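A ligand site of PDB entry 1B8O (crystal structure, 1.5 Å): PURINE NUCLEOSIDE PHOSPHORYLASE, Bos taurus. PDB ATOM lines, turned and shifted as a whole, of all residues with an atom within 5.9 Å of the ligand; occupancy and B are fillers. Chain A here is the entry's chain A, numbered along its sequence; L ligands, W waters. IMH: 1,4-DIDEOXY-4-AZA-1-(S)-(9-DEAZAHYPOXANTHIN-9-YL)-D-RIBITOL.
A ring nitrogen (ND1) of His 257 lies within hydrogen-bond range of an oxygen (O5') of the ligand. OD1 of Asn 243 is in hydrogen-bond range of N7 of the ligand (2.8 Å). An oxygen (O3') of the ligand is in hydrogen-bond range of the side-chain hydroxyl of Tyr 88, at 2.8 Å. An oxygen (O3') of the ligand is in hydrogen-bond range of a ring nitrogen (NE2) of His 86, 3.4 Å away. A nitrogen (N7) of the ligand lies close to the backbone NH of Gly 118 (3.4 Å). N1 of the ligand lies within hydrogen-bond range of OE1 of Glu 201 (2.9 Å). The backbone NH (N) of Met 219 sits at hydrogen-bond distance from an oxygen (O2') of the ligand (2.8 Å).
O of Gly 218 is in hydrogen-bond range of N of Leu 195. The backbone carbonyl oxygen of Asn 243 sits at hydrogen-bond distance from the backbone NH of Gly 119, 2.8 Å away. The backbone carbonyl oxygen (O) of Gly 118 lies within hydrogen-bond range of the backbone NH (N) of Val 217 (2.8 Å). The backbone NH (N) of Met 219 is in hydrogen-bond range of the side-chain hydroxyl (OH) of Tyr 192 (3.3 Å). The backbone NH of Val 245 lies close to the backbone carbonyl oxygen of Gly 119. N of Thr 242 lies within hydrogen-bond range of O of Ala 117 (3.1 Å). OH of Tyr 88 sits at hydrogen-bond distance from ND1 of His 86. The side-chain hydroxyl (OG1) of Thr 242 sits at hydrogen-bond distance from the side-chain amide oxygen (OD1) of Asn 243, 3.0 Å away.
Ser 33 touches the ligand. Ala 116 touches the ligand (O to C1', 3.2 Å). Ala 117 touches the ligand (C to N7, 3.7 Å). Phe 200 touches the ligand (CZ to O5', 3.5 Å). O of Val 217 touches C2 of the ligand, at 3.8 Å. Gly 218 touches the ligand. OG1 of Thr 242 touches C8 of the ligand, 3.7 Å away. CG1 of Val 245 touches O6 of the ligand, at 3.5 Å. Val 260 touches the ligand (CG2 to O5', 3.4 Å). Hydrophobic or aromatic side chains within 4 Å of the ligand: His 86, Tyr 88, Phe 200, Val 217, Met 219, Val 245, His 257 and Val 260. The nearest printed residue that does not touch the ligand is Ser 220 (4.1 Å).
Water W1 lies within hydrogen-bond range of the side-chain carboxylate (OE1) of Glu 201 (2.6 Å) and an oxygen (O6) of the ligand (2.8 Å). Water W2 lies within hydrogen-bond range of the side-chain hydroxyl of Tyr 192, the backbone carbonyl oxygen of Ala 116 and an oxygen (O2') of the ligand.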
ATOM      1  N   SER A  33       2.929  10.262  22.552  1.00  0.00           N
ATOM      2  CA  SER A  33       2.485  11.118  21.445  1.00  0.00           C
ATOM      3  C   SER A  33       1.035  10.872  21.033  1.00  0.00           C
ATOM      4  O   SER A  33       0.680   9.780  20.609  1.00  0.00           O
ATOM      5  CB  SER A  33       3.387  10.913  20.225  1.00  0.00           C
ATOM      6  OG  SER A  33       4.662  11.502  20.408  1.00  0.00           O
ATOM      7  N   VAL A  61       7.611  18.557  22.406  1.00  0.00           N
ATOM      8  CA  VAL A  61       7.122  17.847  21.220  1.00  0.00           C
ATOM      9  C   VAL A  61       5.608  17.966  21.008  1.00  0.00           C
ATOM     10  O   VAL A  61       4.823  17.826  21.953  1.00  0.00           O
ATOM     11  CB  VAL A  61       7.483  16.342  21.306  1.00  0.00           C
ATOM     12  CG1 VAL A  61       6.957  15.605  20.091  1.00  0.00           C
ATOM     13  CG2 VAL A  61       8.990  16.172  21.419  1.00  0.00           C
ATOM     14  N   HIS A  64       2.240  16.487  23.057  1.00  0.00           N
ATOM     15  CA  HIS A  64       2.596  16.327  24.467  1.00  0.00           C
ATOM     16  C   HIS A  64       2.210  17.637  25.147  1.00  0.00           C
ATOM     17  O   HIS A  64       2.889  18.656  24.993  1.00  0.00           O
ATOM     18  CB  HIS A  64       4.104  16.071  24.610  1.00  0.00           C
ATOM     19  CG  HIS A  64       4.546  14.723  24.116  1.00  0.00           C
ATOM     20  ND1 HIS A  64       4.604  14.409  22.776  1.00  0.00           N
ATOM     21  CD2 HIS A  64       4.894  13.592  24.786  1.00  0.00           C
ATOM     22  CE1 HIS A  64       4.979  13.150  22.633  1.00  0.00           C
ATOM     23  NE2 HIS A  64       5.160  12.637  23.838  1.00  0.00           N
ATOM     24  N   HIS A  86      11.922  13.327  25.913  1.00  0.00           N
ATOM     25  CA  HIS A  86      12.734  12.438  25.098  1.00  0.00           C
ATOM     26  C   HIS A  86      14.169  12.911  25.025  1.00  0.00           C
ATOM     27  O   HIS A  86      14.451  14.106  25.106  1.00  0.00           O
ATOM     28  CB  HIS A  86      12.187  12.350  23.670  1.00  0.00           C
ATOM     29  CG  HIS A  86      10.701  12.138  23.596  1.00  0.00           C
ATOM     30  ND1 HIS A  86       9.794  13.158  23.822  1.00  0.00           N
ATOM     31  CD2 HIS A  86       9.977  11.041  23.301  1.00  0.00           C
ATOM     32  CE1 HIS A  86       8.576  12.686  23.668  1.00  0.00           C
ATOM     33  NE2 HIS A  86       8.645  11.408  23.355  1.00  0.00           N
ATOM     34  N   TYR A  88      16.005  12.955  22.438  1.00  0.00           N
ATOM     35  CA  TYR A  88      16.208  13.771  21.247  1.00  0.00           C
ATOM     36  C   TYR A  88      15.860  15.253  21.426  1.00  0.00           C
ATOM     37  O   TYR A  88      16.188  16.069  20.574  1.00  0.00           O
ATOM     38  CB  TYR A  88      15.442  13.184  20.047  1.00  0.00           C
ATOM     39  CG  TYR A  88      13.940  13.130  20.186  1.00  0.00           C
ATOM     40  CD1 TYR A  88      13.172  14.312  20.232  1.00  0.00           C
ATOM     41  CD2 TYR A  88      13.261  11.908  20.240  1.00  0.00           C
ATOM     42  CE1 TYR A  88      11.787  14.271  20.337  1.00  0.00           C
ATOM     43  CE2 TYR A  88      11.872  11.851  20.336  1.00  0.00           C
ATOM     44  CZ  TYR A  88      11.144  13.040  20.386  1.00  0.00           C
ATOM     45  OH  TYR A  88       9.777  12.987  20.513  1.00  0.00           O
ATOM     46  N   ALA A 116       3.606   5.909  21.229  1.00  0.00           N
ATOM     47  CA  ALA A 116       3.213   5.760  19.843  1.00  0.00           C
ATOM     48  C   ALA A 116       4.454   5.093  19.261  1.00  0.00           C
ATOM     49  O   ALA A 116       5.577   5.541  19.519  1.00  0.00           O
ATOM     50  CB  ALA A 116       3.008   7.129  19.209  1.00  0.00           C
ATOM     51  N   ALA A 117       4.287   4.024  18.487  1.00  0.00           N
ATOM     52  CA  ALA A 117       5.446   3.322  17.950  1.00  0.00           C
ATOM     53  C   ALA A 117       5.257   2.865  16.519  1.00  0.00           C
ATOM     54  O   ALA A 117       4.137   2.672  16.058  1.00  0.00           O
ATOM     55  CB  ALA A 117       5.777   2.128  18.817  1.00  0.00           C
ATOM     56  N   GLY A 118       6.373   2.710  15.818  1.00  0.00           N
ATOM     57  CA  GLY A 118       6.327   2.243  14.453  1.00  0.00           C
ATOM     58  C   GLY A 118       6.314   0.729  14.495  1.00  0.00           C
ATOM     59  O   GLY A 118       7.041   0.126  15.281  1.00  0.00           O
ATOM     60  N   GLY A 119       5.480   0.113  13.676  1.00  0.00           N
ATOM     61  CA  GLY A 119       5.405  -1.335  13.658  1.00  0.00           C
ATOM     62  C   GLY A 119       6.465  -1.984  12.797  1.00  0.00           C
ATOM     63  O   GLY A 119       6.644  -1.615  11.636  1.00  0.00           O
ATOM     64  N   TYR A 192       9.633  -4.090  22.301  1.00  0.00           N
ATOM     65  CA  TYR A 192       9.796  -2.688  21.905  1.00  0.00           C
ATOM     66  C   TYR A 192      11.285  -2.344  21.900  1.00  0.00           C
ATOM     67  O   TYR A 192      11.985  -2.600  22.885  1.00  0.00           O
ATOM     68  CB  TYR A 192       9.052  -1.786  22.894  1.00  0.00           C
ATOM     69  CG  TYR A 192       9.249  -0.316  22.661  1.00  0.00           C
ATOM     70  CD1 TYR A 192       8.396   0.408  21.835  1.00  0.00           C
ATOM     71  CD2 TYR A 192      10.271   0.377  23.316  1.00  0.00           C
ATOM     72  CE1 TYR A 192       8.547   1.784  21.649  1.00  0.00           C
ATOM     73  CE2 TYR A 192      10.443   1.749  23.140  1.00  0.00           C
ATOM     74  CZ  TYR A 192       9.563   2.456  22.309  1.00  0.00           C
ATOM     75  OH  TYR A 192       9.682   3.823  22.193  1.00  0.00           O
ATOM     76  N   LEU A 195      15.416   3.628  20.190  1.00  0.00           N
ATOM     77  CA  LEU A 195      16.600   4.231  19.574  1.00  0.00           C
ATOM     78  C   LEU A 195      16.474   5.728  19.856  1.00  0.00           C
ATOM     79  O   LEU A 195      15.430   6.183  20.311  1.00  0.00           O
ATOM     80  CB  LEU A 195      16.686   3.950  18.063  1.00  0.00           C
ATOM     81  CG  LEU A 195      15.434   3.777  17.208  1.00  0.00           C
ATOM     82  CD1 LEU A 195      14.597   5.049  17.227  1.00  0.00           C
ATOM     83  CD2 LEU A 195      15.865   3.424  15.790  1.00  0.00           C
ATOM     84  N   ASN A 199      15.126  11.594  13.836  1.00  0.00           N
ATOM     85  CA  ASN A 199      14.770  11.230  12.472  1.00  0.00           C
ATOM     86  C   ASN A 199      14.109   9.854  12.462  1.00  0.00           C
ATOM     87  O   ASN A 199      14.362   9.032  13.337  1.00  0.00           O
ATOM     88  CB  ASN A 199      16.013  11.202  11.588  1.00  0.00           C
ATOM     89  CG  ASN A 199      17.012  10.160  12.038  1.00  0.00           C
ATOM     90  OD1 ASN A 199      17.839  10.413  12.900  1.00  0.00           O
ATOM     91  ND2 ASN A 199      16.948   8.960  11.446  1.00  0.00           N
ATOM     92  N   PHE A 200      13.241   9.615  11.486  1.00  0.00           N
ATOM     93  CA  PHE A 200      12.604   8.312  11.380  1.00  0.00           C
ATOM     94  C   PHE A 200      13.621   7.374  10.704  1.00  0.00           C
ATOM     95  O   PHE A 200      14.552   7.840  10.039  1.00  0.00           O
ATOM     96  CB  PHE A 200      11.308   8.413  10.570  1.00  0.00           C
ATOM     97  CG  PHE A 200      10.159   9.033  11.334  1.00  0.00           C
ATOM     98  CD1 PHE A 200       9.606   8.386  12.431  1.00  0.00           C
ATOM     99  CD2 PHE A 200       9.637  10.273  10.963  1.00  0.00           C
ATOM    100  CE1 PHE A 200       8.551   8.957  13.149  1.00  0.00           C
ATOM    101  CE2 PHE A 200       8.585  10.841  11.672  1.00  0.00           C
ATOM    102  CZ  PHE A 200       8.046  10.184  12.767  1.00  0.00           C
ATOM    103  N   GLU A 201      13.443   6.075  10.875  1.00  0.00           N
ATOM    104  CA  GLU A 201      14.391   5.081  10.349  1.00  0.00           C
ATOM    105  C   GLU A 201      14.506   4.891   8.842  1.00  0.00           C
ATOM    106  O   GLU A 201      13.571   5.159   8.094  1.00  0.00           O
ATOM    107  CB  GLU A 201      14.086   3.713  10.980  1.00  0.00           C
ATOM    108  CG  GLU A 201      14.106   3.689  12.507  1.00  0.00           C
ATOM    109  CD  GLU A 201      12.935   4.429  13.116  1.00  0.00           C
ATOM    110  OE1 GLU A 201      11.808   4.323  12.577  1.00  0.00           O
ATOM    111  OE2 GLU A 201      13.130   5.095  14.146  1.00  0.00           O
ATOM    112  N   VAL A 217       9.135  -0.001  17.186  1.00  0.00           N
ATOM    113  CA  VAL A 217      10.262   0.900  17.437  1.00  0.00           C
ATOM    114  C   VAL A 217       9.822   2.295  17.859  1.00  0.00           C
ATOM    115  O   VAL A 217       8.853   2.856  17.338  1.00  0.00           O
ATOM    116  CB  VAL A 217      11.170   1.000  16.193  1.00  0.00           C
ATOM    117  CG1 VAL A 217      10.349   1.441  14.977  1.00  0.00           C
ATOM    118  CG2 VAL A 217      12.317   1.949  16.447  1.00  0.00           C
ATOM    119  N   GLY A 218      10.555   2.860  18.823  1.00  0.00           N
ATOM    120  CA  GLY A 218      10.247   4.184  19.326  1.00  0.00           C
ATOM    121  C   GLY A 218      11.468   4.848  19.929  1.00  0.00           C
ATOM    122  O   GLY A 218      12.541   4.246  20.018  1.00  0.00           O
ATOM    123  N   MET A 219      11.303   6.096  20.360  1.00  0.00           N
ATOM    124  CA  MET A 219      12.380   6.893  20.934  1.00  0.00           C
ATOM    125  C   MET A 219      12.143   7.285  22.388  1.00  0.00           C
ATOM    126  O   MET A 219      12.610   8.328  22.842  1.00  0.00           O
ATOM    127  CB  MET A 219      12.566   8.179  20.109  1.00  0.00           C
ATOM    128  CG  MET A 219      12.602   7.958  18.601  1.00  0.00           C
ATOM    129  SD  MET A 219      12.283   9.486  17.669  1.00  0.00           S
ATOM    130  CE  MET A 219      12.392   8.869  15.964  1.00  0.00           C
ATOM    131  N   SER A 220      11.426   6.442  23.127  1.00  0.00           N
ATOM    132  CA  SER A 220      11.108   6.749  24.530  1.00  0.00           C
ATOM    133  C   SER A 220      10.864   5.477  25.325  1.00  0.00           C
ATOM    134  O   SER A 220      11.298   4.389  24.943  1.00  0.00           O
ATOM    135  CB  SER A 220       9.831   7.578  24.583  1.00  0.00           C
ATOM    136  OG  SER A 220       8.708   6.789  24.203  1.00  0.00           O
ATOM    137  N   THR A 242       1.151   3.332  15.538  1.00  0.00           N
ATOM    138  CA  THR A 242       0.674   4.506  14.798  1.00  0.00           C
ATOM    139  C   THR A 242       1.032   4.527  13.310  1.00  0.00           C
ATOM    140  O   THR A 242       0.475   5.316  12.556  1.00  0.00           O
ATOM    141  CB  THR A 242       1.205   5.806  15.442  1.00  0.00           C
ATOM    142  OG1 THR A 242       2.625   5.731  15.576  1.00  0.00           O
ATOM    143  CG2 THR A 242       0.595   5.996  16.805  1.00  0.00           C
ATOM    144  N   ASN A 243       1.974   3.681  12.913  1.00  0.00           N
ATOM    145  CA  ASN A 243       2.413   3.635  11.529  1.00  0.00           C
ATOM    146  C   ASN A 243       3.253   2.395  11.317  1.00  0.00           C
ATOM    147  O   ASN A 243       3.849   1.889  12.253  1.00  0.00           O
ATOM    148  CB  ASN A 243       3.238   4.888  11.184  1.00  0.00           C
ATOM    149  CG  ASN A 243       4.494   5.006  12.038  1.00  0.00           C
ATOM    150  OD1 ASN A 243       4.424   5.313  13.227  1.00  0.00           O
ATOM    151  ND2 ASN A 243       5.653   4.774  11.429  1.00  0.00           N
ATOM    152  N   VAL A 245       6.491   1.000   9.767  1.00  0.00           N
ATOM    153  CA  VAL A 245       7.768   1.483   9.256  1.00  0.00           C
ATOM    154  C   VAL A 245       8.008   0.988   7.841  1.00  0.00           C
ATOM    155  O   VAL A 245       7.732  -0.173   7.521  1.00  0.00           O
ATOM    156  CB  VAL A 245       8.926   1.026  10.166  1.00  0.00           C
ATOM    157  CG1 VAL A 245       8.704   1.536  11.584  1.00  0.00           C
ATOM    158  CG2 VAL A 245       9.020  -0.469  10.167  1.00  0.00           C
ATOM    159  N   ALA A 255       7.266   7.953   6.911  1.00  0.00           N
ATOM    160  CA  ALA A 255       6.830   8.220   8.276  1.00  0.00           C
ATOM    161  C   ALA A 255       6.785   9.712   8.548  1.00  0.00           C
ATOM    162  O   ALA A 255       7.624  10.466   8.063  1.00  0.00           O
ATOM    163  CB  ALA A 255       7.784   7.538   9.256  1.00  0.00           C
ATOM    164  N   ASN A 256       5.786  10.142   9.306  1.00  0.00           N
ATOM    165  CA  ASN A 256       5.617  11.543   9.659  1.00  0.00           C
ATOM    166  C   ASN A 256       4.811  11.702  10.949  1.00  0.00           C
ATOM    167  O   ASN A 256       3.820  11.005  11.166  1.00  0.00           O
ATOM    168  CB  ASN A 256       4.941  12.300   8.510  1.00  0.00           C
ATOM    169  CG  ASN A 256       3.531  11.827   8.251  1.00  0.00           C
ATOM    170  OD1 ASN A 256       2.579  12.418   8.745  1.00  0.00           O
ATOM    171  ND2 ASN A 256       3.401  10.750   7.473  1.00  0.00           N
ATOM    172  N   HIS A 257       5.266  12.609  11.800  1.00  0.00           N
ATOM    173  CA  HIS A 257       4.625  12.851  13.086  1.00  0.00           C
ATOM    174  C   HIS A 257       3.138  13.207  12.996  1.00  0.00           C
ATOM    175  O   HIS A 257       2.345  12.774  13.835  1.00  0.00           O
ATOM    176  CB  HIS A 257       5.366  13.967  13.827  1.00  0.00           C
ATOM    177  CG  HIS A 257       5.070  14.030  15.290  1.00  0.00           C
ATOM    178  ND1 HIS A 257       5.182  12.935  16.120  1.00  0.00           N
ATOM    179  CD2 HIS A 257       4.678  15.057  16.077  1.00  0.00           C
ATOM    180  CE1 HIS A 257       4.865  13.285  17.359  1.00  0.00           C
ATOM    181  NE2 HIS A 257       4.563  14.572  17.363  1.00  0.00           N
ATOM    182  N   VAL A 260       1.165  10.270  12.851  1.00  0.00           N
ATOM    183  CA  VAL A 260       1.327   9.531  14.093  1.00  0.00           C
ATOM    184  C   VAL A 260       0.319  10.107  15.082  1.00  0.00           C
ATOM    185  O   VAL A 260      -0.364   9.368  15.800  1.00  0.00           O
ATOM    186  CB  VAL A 260       2.762   9.693  14.677  1.00  0.00           C
ATOM    187  CG1 VAL A 260       2.781   9.295  16.139  1.00  0.00           C
ATOM    188  CG2 VAL A 260       3.740   8.844  13.885  1.00  0.00           C
HETATM  189  O5' IMH L   1       6.159  10.264  15.734  1.00  0.00           O
HETATM  190  C5' IMH L   1       7.398  10.490  16.428  1.00  0.00           C
HETATM  191  C4' IMH L   1       7.386  10.343  17.983  1.00  0.00           C
HETATM  192  N4' IMH L   1       6.541   9.166  18.201  1.00  0.00           N
HETATM  193  C3' IMH L   1       8.710   9.985  18.712  1.00  0.00           C
HETATM  194  O3' IMH L   1       8.762  10.449  20.093  1.00  0.00           O
HETATM  195  C2' IMH L   1       8.765   8.405  18.703  1.00  0.00           C
HETATM  196  O2' IMH L   1       9.141   7.845  19.975  1.00  0.00           O
HETATM  197  C1' IMH L   1       7.332   7.951  18.337  1.00  0.00           C
HETATM  198  C9  IMH L   1       7.229   7.101  16.954  1.00  0.00           C
HETATM  199  C8  IMH L   1       6.087   6.835  16.292  1.00  0.00           C
HETATM  200  N7  IMH L   1       6.382   6.080  15.105  1.00  0.00           N
HETATM  201  C5  IMH L   1       7.787   5.942  15.140  1.00  0.00           C
HETATM  202  C6  IMH L   1       8.606   5.220  14.144  1.00  0.00           C
HETATM  203  O6  IMH L   1       8.243   4.696  13.085  1.00  0.00           O
HETATM  204  N1  IMH L   1       9.964   5.288  14.545  1.00  0.00           N
HETATM  205  C2  IMH L   1      10.463   5.904  15.711  1.00  0.00           C
HETATM  206  N3  IMH L   1       9.638   6.528  16.544  1.00  0.00           N
HETATM  207  C4  IMH L   1       8.324   6.519  16.222  1.00  0.00           C
HETATM  208  O   HOH W   1       9.912   4.863  10.830  1.00  0.00           O
HETATM  209  O   HOH W   2       7.668   5.134  21.132  1.00  0.00           O
